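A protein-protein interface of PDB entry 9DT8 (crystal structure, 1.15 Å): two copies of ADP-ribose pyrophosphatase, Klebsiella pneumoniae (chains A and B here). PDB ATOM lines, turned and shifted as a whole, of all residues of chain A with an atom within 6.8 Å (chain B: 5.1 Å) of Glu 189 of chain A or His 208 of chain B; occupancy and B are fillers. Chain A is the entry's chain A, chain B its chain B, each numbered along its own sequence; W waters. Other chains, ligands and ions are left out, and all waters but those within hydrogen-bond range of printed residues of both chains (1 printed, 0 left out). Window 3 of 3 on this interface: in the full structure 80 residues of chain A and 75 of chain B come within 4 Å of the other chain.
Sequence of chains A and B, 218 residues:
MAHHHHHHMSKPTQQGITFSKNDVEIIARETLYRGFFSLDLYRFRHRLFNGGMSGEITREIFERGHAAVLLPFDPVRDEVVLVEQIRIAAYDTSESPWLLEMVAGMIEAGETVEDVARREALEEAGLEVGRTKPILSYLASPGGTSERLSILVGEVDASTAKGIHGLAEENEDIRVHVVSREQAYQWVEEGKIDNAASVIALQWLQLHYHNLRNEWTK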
ATOM      1  N   ALA A 184     -27.347 -25.292  -6.007  1.00  0.00           N
ATOM      2  CA  ALA A 184     -26.069 -24.684  -5.661  1.00  0.00           C
ATOM      3  C   ALA A 184     -25.785 -24.822  -4.172  1.00  0.00           C
ATOM      4  O   ALA A 184     -24.663 -25.147  -3.768  1.00  0.00           O
ATOM      5  CB  ALA A 184     -26.055 -23.220  -6.077  1.00  0.00           C
ATOM      6  N   TYR A 185     -26.797 -24.603  -3.343  1.00  0.00           N
ATOM      7  CA  TYR A 185     -26.608 -24.744  -1.909  1.00  0.00           C
ATOM      8  C   TYR A 185     -26.345 -26.194  -1.523  1.00  0.00           C
ATOM      9  O   TYR A 185     -25.483 -26.476  -0.690  1.00  0.00           O
ATOM     10  CB  TYR A 185     -27.790 -24.157  -1.139  1.00  0.00           C
ATOM     11  CG  TYR A 185     -27.566 -24.313   0.334  1.00  0.00           C
ATOM     12  CD1 TYR A 185     -26.604 -23.561   1.006  1.00  0.00           C
ATOM     13  CD2 TYR A 185     -28.255 -25.278   1.039  1.00  0.00           C
ATOM     14  CE1 TYR A 185     -26.380 -23.755   2.360  1.00  0.00           C
ATOM     15  CE2 TYR A 185     -28.032 -25.479   2.370  1.00  0.00           C
ATOM     16  CZ  TYR A 185     -27.096 -24.726   3.027  1.00  0.00           C
ATOM     17  OH  TYR A 185     -26.893 -24.940   4.366  1.00  0.00           O
ATOM     18  N   GLN A 186     -27.068 -27.138  -2.116  1.00  0.00           N
ATOM     19  CA  GLN A 186     -26.755 -28.530  -1.821  1.00  0.00           C
ATOM     20  C   GLN A 186     -25.329 -28.879  -2.239  1.00  0.00           C
ATOM     21  O   GLN A 186     -24.662 -29.667  -1.557  1.00  0.00           O
ATOM     22  CB  GLN A 186     -27.791 -29.472  -2.431  1.00  0.00           C
ATOM     23  CG  GLN A 186     -29.155 -29.417  -1.728  1.00  0.00           C
ATOM     24  CD  GLN A 186     -29.068 -29.628  -0.215  1.00  0.00           C
ATOM     25  OE1 GLN A 186     -28.324 -30.488   0.263  1.00  0.00           O
ATOM     26  NE2 GLN A 186     -29.815 -28.825   0.543  1.00  0.00           N
ATOM     27  N   TRP A 187     -24.824 -28.284  -3.317  1.00  0.00           N
ATOM     28  CA  TRP A 187     -23.432 -28.520  -3.690  1.00  0.00           C
ATOM     29  C   TRP A 187     -22.450 -27.957  -2.655  1.00  0.00           C
ATOM     30  O   TRP A 187     -21.362 -28.508  -2.467  1.00  0.00           O
ATOM     31  CB  TRP A 187     -23.178 -27.955  -5.084  1.00  0.00           C
ATOM     32  CG  TRP A 187     -23.658 -28.825  -6.203  1.00  0.00           C
ATOM     33  CD1 TRP A 187     -24.040 -30.121  -6.122  1.00  0.00           C
ATOM     34  CD2 TRP A 187     -23.792 -28.443  -7.571  1.00  0.00           C
ATOM     35  NE1 TRP A 187     -24.395 -30.590  -7.367  1.00  0.00           N
ATOM     36  CE2 TRP A 187     -24.265 -29.567  -8.271  1.00  0.00           C
ATOM     37  CE3 TRP A 187     -23.556 -27.262  -8.272  1.00  0.00           C
ATOM     38  CZ2 TRP A 187     -24.496 -29.544  -9.638  1.00  0.00           C
ATOM     39  CZ3 TRP A 187     -23.783 -27.240  -9.622  1.00  0.00           C
ATOM     40  CH2 TRP A 187     -24.245 -28.371 -10.293  1.00  0.00           C
ATOM     41  N   VAL A 188     -22.791 -26.859  -1.994  1.00  0.00           N
ATOM     42  CA  VAL A 188     -21.992 -26.404  -0.859  1.00  0.00           C
ATOM     43  C   VAL A 188     -22.011 -27.460   0.244  1.00  0.00           C
ATOM     44  O   VAL A 188     -20.967 -27.848   0.773  1.00  0.00           O
ATOM     45  CB  VAL A 188     -22.497 -25.039  -0.355  1.00  0.00           C
ATOM     46  CG1 VAL A 188     -21.862 -24.691   1.004  1.00  0.00           C
ATOM     47  CG2 VAL A 188     -22.205 -23.958  -1.376  1.00  0.00           C
ATOM     48  N   GLU A 189     -23.200 -27.939   0.598  1.00  0.00           N
ATOM     49  CA  GLU A 189     -23.306 -28.943   1.651  1.00  0.00           C
ATOM     50  C   GLU A 189     -22.504 -30.195   1.314  1.00  0.00           C
ATOM     51  O   GLU A 189     -21.892 -30.801   2.199  1.00  0.00           O
ATOM     52  CB  GLU A 189     -24.778 -29.279   1.881  1.00  0.00           C
ATOM     53  CG  GLU A 189     -25.539 -28.168   2.605  1.00  0.00           C
ATOM     54  CD  GLU A 189     -25.219 -28.111   4.108  1.00  0.00           C
ATOM     55  OE1 GLU A 189     -24.155 -27.544   4.491  1.00  0.00           O
ATOM     56  OE2 GLU A 189     -26.025 -28.648   4.906  1.00  0.00           O
ATOM     57  N   GLU A 190     -22.493 -30.592   0.040  1.00  0.00           N
ATOM     58  CA  GLU A 190     -21.821 -31.803  -0.405  1.00  0.00           C
ATOM     59  C   GLU A 190     -20.331 -31.618  -0.648  1.00  0.00           C
ATOM     60  O   GLU A 190     -19.632 -32.600  -0.906  1.00  0.00           O
ATOM     61  CB  GLU A 190     -22.466 -32.290  -1.708  1.00  0.00           C
ATOM     62  CG  GLU A 190     -23.931 -32.712  -1.551  1.00  0.00           C
ATOM     63  CD  GLU A 190     -24.614 -33.046  -2.869  1.00  0.00           C
ATOM     64  OE1 GLU A 190     -23.968 -32.958  -3.925  1.00  0.00           O
ATOM     65  OE2 GLU A 190     -25.804 -33.395  -2.843  1.00  0.00           O
ATOM     66  N   GLY A 191     -19.830 -30.398  -0.611  1.00  0.00           N
ATOM     67  CA  GLY A 191     -18.438 -30.134  -0.893  1.00  0.00           C
ATOM     68  C   GLY A 191     -18.077 -29.959  -2.348  1.00  0.00           C
ATOM     69  O   GLY A 191     -16.886 -29.834  -2.654  1.00  0.00           O
ATOM     70  N   LYS A 192     -19.063 -29.931  -3.247  1.00  0.00           N
ATOM     71  CA  LYS A 192     -18.815 -29.715  -4.667  1.00  0.00           C
ATOM     72  C   LYS A 192     -18.565 -28.251  -4.992  1.00  0.00           C
ATOM     73  O   LYS A 192     -18.005 -27.954  -6.055  1.00  0.00           O
ATOM     74  CB  LYS A 192     -19.986 -30.267  -5.478  1.00  0.00           C
ATOM     75  CG  LYS A 192     -20.100 -31.792  -5.426  1.00  0.00           C
ATOM     76  CD  LYS A 192     -21.155 -32.304  -6.385  1.00  0.00           C
ATOM     77  CE  LYS A 192     -21.199 -33.827  -6.421  1.00  0.00           C
ATOM     78  NZ  LYS A 192     -21.837 -34.438  -5.210  1.00  0.00           N
ATOM     79  N   ILE A 193     -19.007 -27.346  -4.128  1.00  0.00           N
ATOM     80  CA  ILE A 193     -18.632 -25.942  -4.137  1.00  0.00           C
ATOM     81  C   ILE A 193     -17.952 -25.705  -2.795  1.00  0.00           C
ATOM     82  O   ILE A 193     -18.572 -25.901  -1.746  1.00  0.00           O
ATOM     83  CB  ILE A 193     -19.843 -25.018  -4.337  1.00  0.00           C
ATOM     84  CG1 ILE A 193     -20.435 -25.195  -5.726  1.00  0.00           C
ATOM     85  CG2 ILE A 193     -19.416 -23.591  -4.115  1.00  0.00           C
ATOM     86  CD1 ILE A 193     -21.719 -24.438  -5.911  1.00  0.00           C
ATOM     87  N   GLN A 203     -24.242 -19.397   1.272  1.00  0.00           N
ATOM     88  CA  GLN A 203     -24.857 -19.498   2.587  1.00  0.00           C
ATOM     89  C   GLN A 203     -25.648 -18.223   2.905  1.00  0.00           C
ATOM     90  O   GLN A 203     -26.750 -18.303   3.449  1.00  0.00           O
ATOM     91  CB  GLN A 203     -23.822 -19.838   3.673  1.00  0.00           C
ATOM     92  CG  GLN A 203     -23.248 -21.276   3.609  1.00  0.00           C
ATOM     93  CD  GLN A 203     -22.451 -21.675   4.852  1.00  0.00           C
ATOM     94  OE1 GLN A 203     -22.640 -22.763   5.397  1.00  0.00           O
ATOM     95  NE2 GLN A 203     -21.547 -20.808   5.286  1.00  0.00           N
ATOM     96  N   LEU B 136     -17.625 -27.766   7.075  1.00  0.00           N
ATOM     97  CA  LEU B 136     -17.286 -27.652   5.658  1.00  0.00           C
ATOM     98  C   LEU B 136     -15.765 -27.552   5.606  1.00  0.00           C
ATOM     99  O   LEU B 136     -15.166 -27.036   6.551  1.00  0.00           O
ATOM    100  CB  LEU B 136     -17.884 -26.372   5.049  1.00  0.00           C
ATOM    101  CG  LEU B 136     -19.408 -26.237   4.988  1.00  0.00           C
ATOM    102  CD1 LEU B 136     -19.843 -24.826   4.539  1.00  0.00           C
ATOM    103  CD2 LEU B 136     -20.006 -27.297   4.083  1.00  0.00           C
ATOM    104  N   TRP B 204     -23.088 -21.181   8.761  1.00  0.00           N
ATOM    105  CA  TRP B 204     -23.469 -22.572   8.881  1.00  0.00           C
ATOM    106  C   TRP B 204     -24.273 -22.795  10.151  1.00  0.00           C
ATOM    107  O   TRP B 204     -25.322 -23.434  10.131  1.00  0.00           O
ATOM    108  CB  TRP B 204     -22.247 -23.492   8.863  1.00  0.00           C
ATOM    109  CG  TRP B 204     -22.581 -24.936   8.982  1.00  0.00           C
ATOM    110  CD1 TRP B 204     -22.759 -25.822   7.965  1.00  0.00           C
ATOM    111  CD2 TRP B 204     -22.759 -25.687  10.190  1.00  0.00           C
ATOM    112  NE1 TRP B 204     -23.024 -27.073   8.460  1.00  0.00           N
ATOM    113  CE2 TRP B 204     -23.041 -27.015   9.825  1.00  0.00           C
ATOM    114  CE3 TRP B 204     -22.710 -25.363  11.555  1.00  0.00           C
ATOM    115  CZ2 TRP B 204     -23.284 -28.009  10.760  1.00  0.00           C
ATOM    116  CZ3 TRP B 204     -22.952 -26.368  12.478  1.00  0.00           C
ATOM    117  CH2 TRP B 204     -23.239 -27.664  12.078  1.00  0.00           C
ATOM    118  N   LEU B 205     -23.812 -22.237  11.259  1.00  0.00           N
ATOM    119  CA  LEU B 205     -24.521 -22.423  12.513  1.00  0.00           C
ATOM    120  C   LEU B 205     -25.916 -21.834  12.443  1.00  0.00           C
ATOM    121  O   LEU B 205     -26.871 -22.413  12.974  1.00  0.00           O
ATOM    122  CB  LEU B 205     -23.698 -21.816  13.650  1.00  0.00           C
ATOM    123  CG  LEU B 205     -24.286 -22.022  15.051  1.00  0.00           C
ATOM    124  CD1 LEU B 205     -24.420 -23.480  15.411  1.00  0.00           C
ATOM    125  CD2 LEU B 205     -23.452 -21.249  16.076  1.00  0.00           C
ATOM    126  N   GLN B 206     -26.068 -20.679  11.806  1.00  0.00           N
ATOM    127  CA  GLN B 206     -27.397 -20.093  11.687  1.00  0.00           C
ATOM    128  C   GLN B 206     -28.325 -20.979  10.856  1.00  0.00           C
ATOM    129  O   GLN B 206     -29.532 -20.985  11.087  1.00  0.00           O
ATOM    130  CB  GLN B 206     -27.262 -18.674  11.129  1.00  0.00           C
ATOM    131  CG  GLN B 206     -28.389 -17.703  11.461  1.00  0.00           C
ATOM    132  CD  GLN B 206     -28.503 -17.354  12.944  1.00  0.00           C
ATOM    133  OE1 GLN B 206     -27.654 -17.715  13.753  1.00  0.00           O
ATOM    134  NE2 GLN B 206     -29.571 -16.649  13.301  1.00  0.00           N
ATOM    135  N   LEU B 207     -27.781 -21.727   9.906  1.00  0.00           N
ATOM    136  CA  LEU B 207     -28.558 -22.624   9.075  1.00  0.00           C
ATOM    137  C   LEU B 207     -28.810 -23.974   9.730  1.00  0.00           C
ATOM    138  O   LEU B 207     -29.707 -24.695   9.291  1.00  0.00           O
ATOM    139  CB  LEU B 207     -27.838 -22.834   7.740  1.00  0.00           C
ATOM    140  CG  LEU B 207     -27.919 -21.622   6.806  1.00  0.00           C
ATOM    141  CD1 LEU B 207     -26.833 -21.632   5.746  1.00  0.00           C
ATOM    142  CD2 LEU B 207     -29.289 -21.537   6.167  1.00  0.00           C
ATOM    143  N   HIS B 208     -28.054 -24.357  10.754  1.00  0.00           N
ATOM    144  CA  HIS B 208     -28.111 -25.707  11.295  1.00  0.00           C
ATOM    145  C   HIS B 208     -28.340 -25.802  12.796  1.00  0.00           C
ATOM    146  O   HIS B 208     -28.458 -26.918  13.316  1.00  0.00           O
ATOM    147  CB  HIS B 208     -26.826 -26.492  10.958  1.00  0.00           C
ATOM    148  CG  HIS B 208     -26.658 -26.744   9.504  1.00  0.00           C
ATOM    149  ND1 HIS B 208     -26.022 -25.853   8.668  1.00  0.00           N
ATOM    150  CD2 HIS B 208     -27.047 -27.777   8.725  1.00  0.00           C
ATOM    151  CE1 HIS B 208     -26.046 -26.314   7.435  1.00  0.00           C
ATOM    152  NE2 HIS B 208     -26.648 -27.485   7.441  1.00  0.00           N
ATOM    153  N   TYR B 209     -28.462 -24.680  13.497  1.00  0.00           N
ATOM    154  CA  TYR B 209     -28.468 -24.749  14.958  1.00  0.00           C
ATOM    155  C   TYR B 209     -29.651 -25.528  15.517  1.00  0.00           C
ATOM    156  O   TYR B 209     -29.518 -26.169  16.556  1.00  0.00           O
ATOM    157  CB  TYR B 209     -28.425 -23.353  15.596  1.00  0.00           C
ATOM    158  CG  TYR B 209     -29.683 -22.545  15.407  1.00  0.00           C
ATOM    159  CD1 TYR B 209     -29.865 -21.756  14.290  1.00  0.00           C
ATOM    160  CD2 TYR B 209     -30.689 -22.555  16.368  1.00  0.00           C
ATOM    161  CE1 TYR B 209     -31.016 -20.998  14.116  1.00  0.00           C
ATOM    162  CE2 TYR B 209     -31.845 -21.808  16.196  1.00  0.00           C
ATOM    163  CZ  TYR B 209     -31.998 -21.026  15.068  1.00  0.00           C
ATOM    164  OH  TYR B 209     -33.136 -20.269  14.882  1.00  0.00           O
ATOM    165  N   HIS B 210     -30.814 -25.467  14.880  1.00  0.00           N
ATOM    166  CA  HIS B 210     -31.977 -26.126  15.466  1.00  0.00           C
ATOM    167  C   HIS B 210     -31.755 -27.629  15.555  1.00  0.00           C
ATOM    168  O   HIS B 210     -31.940 -28.249  16.613  1.00  0.00           O
ATOM    169  CB  HIS B 210     -33.202 -25.812  14.621  1.00  0.00           C
ATOM    170  CG  HIS B 210     -34.451 -26.450  15.122  1.00  0.00           C
ATOM    171  ND1 HIS B 210     -35.210 -25.906  16.135  1.00  0.00           N
ATOM    172  CD2 HIS B 210     -35.070 -27.597  14.761  1.00  0.00           C
ATOM    173  CE1 HIS B 210     -36.248 -26.687  16.371  1.00  0.00           C
ATOM    174  NE2 HIS B 210     -36.188 -27.721  15.549  1.00  0.00           N
ATOM    175  N   ASN B 211     -31.325 -28.229  14.447  1.00  0.00           N
ATOM    176  CA  ASN B 211     -31.059 -29.661  14.444  1.00  0.00           C
ATOM    177  C   ASN B 211     -29.855 -30.000  15.311  1.00  0.00           C
ATOM    178  O   ASN B 211     -29.850 -31.030  15.993  1.00  0.00           O
ATOM    179  CB  ASN B 211     -30.845 -30.144  13.011  1.00  0.00           C
ATOM    180  CG  ASN B 211     -32.131 -30.177  12.212  1.00  0.00           C
ATOM    181  OD1 ASN B 211     -33.233 -30.190  12.770  1.00  0.00           O
ATOM    182  ND2 ASN B 211     -32.000 -30.218  10.894  1.00  0.00           N
ATOM    183  N   LEU B 212     -28.820 -29.158  15.286  1.00  0.00           N
ATOM    184  CA  LEU B 212     -27.632 -29.455  16.080  1.00  0.00           C
ATOM    185  C   LEU B 212     -27.942 -29.437  17.569  1.00  0.00           C
ATOM    186  O   LEU B 212     -27.502 -30.322  18.317  1.00  0.00           O
ATOM    187  CB  LEU B 212     -26.522 -28.462  15.748  1.00  0.00           C
ATOM    188  CG  LEU B 212     -25.211 -28.682  16.502  1.00  0.00           C
ATOM    189  CD1 LEU B 212     -24.612 -30.072  16.240  1.00  0.00           C
ATOM    190  CD2 LEU B 212     -24.241 -27.593  16.118  1.00  0.00           C
ATOM    191  N   ARG B 213     -28.689 -28.430  18.025  1.00  0.00           N
ATOM    192  CA  ARG B 213     -29.039 -28.375  19.439  1.00  0.00           C
ATOM    193  C   ARG B 213     -29.901 -29.564  19.826  1.00  0.00           C
ATOM    194  O   ARG B 213     -29.735 -30.127  20.908  1.00  0.00           O
ATOM    195  CB  ARG B 213     -29.742 -27.063  19.767  1.00  0.00           C
ATOM    196  CG  ARG B 213     -28.859 -25.825  19.679  1.00  0.00           C
ATOM    197  CD  ARG B 213     -29.558 -24.609  20.220  1.00  0.00           C
ATOM    198  NE  ARG B 213     -29.640 -24.678  21.675  1.00  0.00           N
ATOM    199  CZ  ARG B 213     -30.477 -23.975  22.427  1.00  0.00           C
ATOM    200  NH1 ARG B 213     -31.409 -23.203  21.894  1.00  0.00           N
ATOM    201  NH2 ARG B 213     -30.369 -24.040  23.748  1.00  0.00           N
HETATM  202  O   HOH W   1     -22.733 -29.268   6.521  1.00  0.00           O
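Among the printed residues, merely in contact across the chains: Tyr 185 of chain A with His 208 of chain B, Val 188 of chain A with Leu 136 of chain B, Gln 203 of chain A with Trp 204 of chain B, Gln 203 of chain A with Leu 136 of chain B and Tyr 185 of chain A with Leu 207 of chain B.
No position is printed for both chains.
Of the 6 pairs that touch across the chains among the printed residues, none has its exchanged pair printed and touching as well.
Glu 189 of chain A touches one residue of chain B.
Printed residues of chain A within 4 Å of His 208 of chain B: Tyr 185 and Glu 189.
Of the printed residues of chain A, Trp 204 of chain B touches Gln 203.
Of the printed residues of chain B, Tyr 185 of chain A touches Leu 207 (3.6 Å) and His 208 (3.5 Å).
Of the printed residues of chain B, Gln 203 of chain A touches Leu 136 (3.6 Å) and Trp 204 (3.6 Å).
His 210 of chain B touches none of the printed residues of chain A.
The nearest printed residue of chain B that does not touch Gln 203 of chain A is Leu 207 of chain B (4.05 Å).
Printed residues of chain B that touch a printed residue of chain A: Leu 136, Trp 204, Leu 207 and His 208.
Hydrophobic or aromatic side chains of chain B within 4 Å of the printed part of chain A: Leu 136, Trp 204, Leu 207 and His 208.
Hydrophobic or aromatic side chains of chain A that line the printed part of chain B: Tyr 185.
Among the printed residues, 6 pairs touch across the chains.
Among the printed residues, no Asp or Glu carboxylate lies within 4 Å of a Lys or Arg side-chain nitrogen of the other chain.
Water W1 lies within hydrogen-bond range of the indole nitrogen (NE1) of Trp 204 of chain B (2.9 Å) and the side-chain carboxylate (OE1) of Glu 189 of chain A (3.0 Å).
The backbone carbonyl oxygen (O) of Trp 204 of chain B sits at hydrogen-bond distance from a ring nitrogen (ND1) of His 208 of chain B, 2.9 Å away.
OE2 of Glu 189 of chain A lies within hydrogen-bond range of NE2 of His 208 of chain B (2.9 Å).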
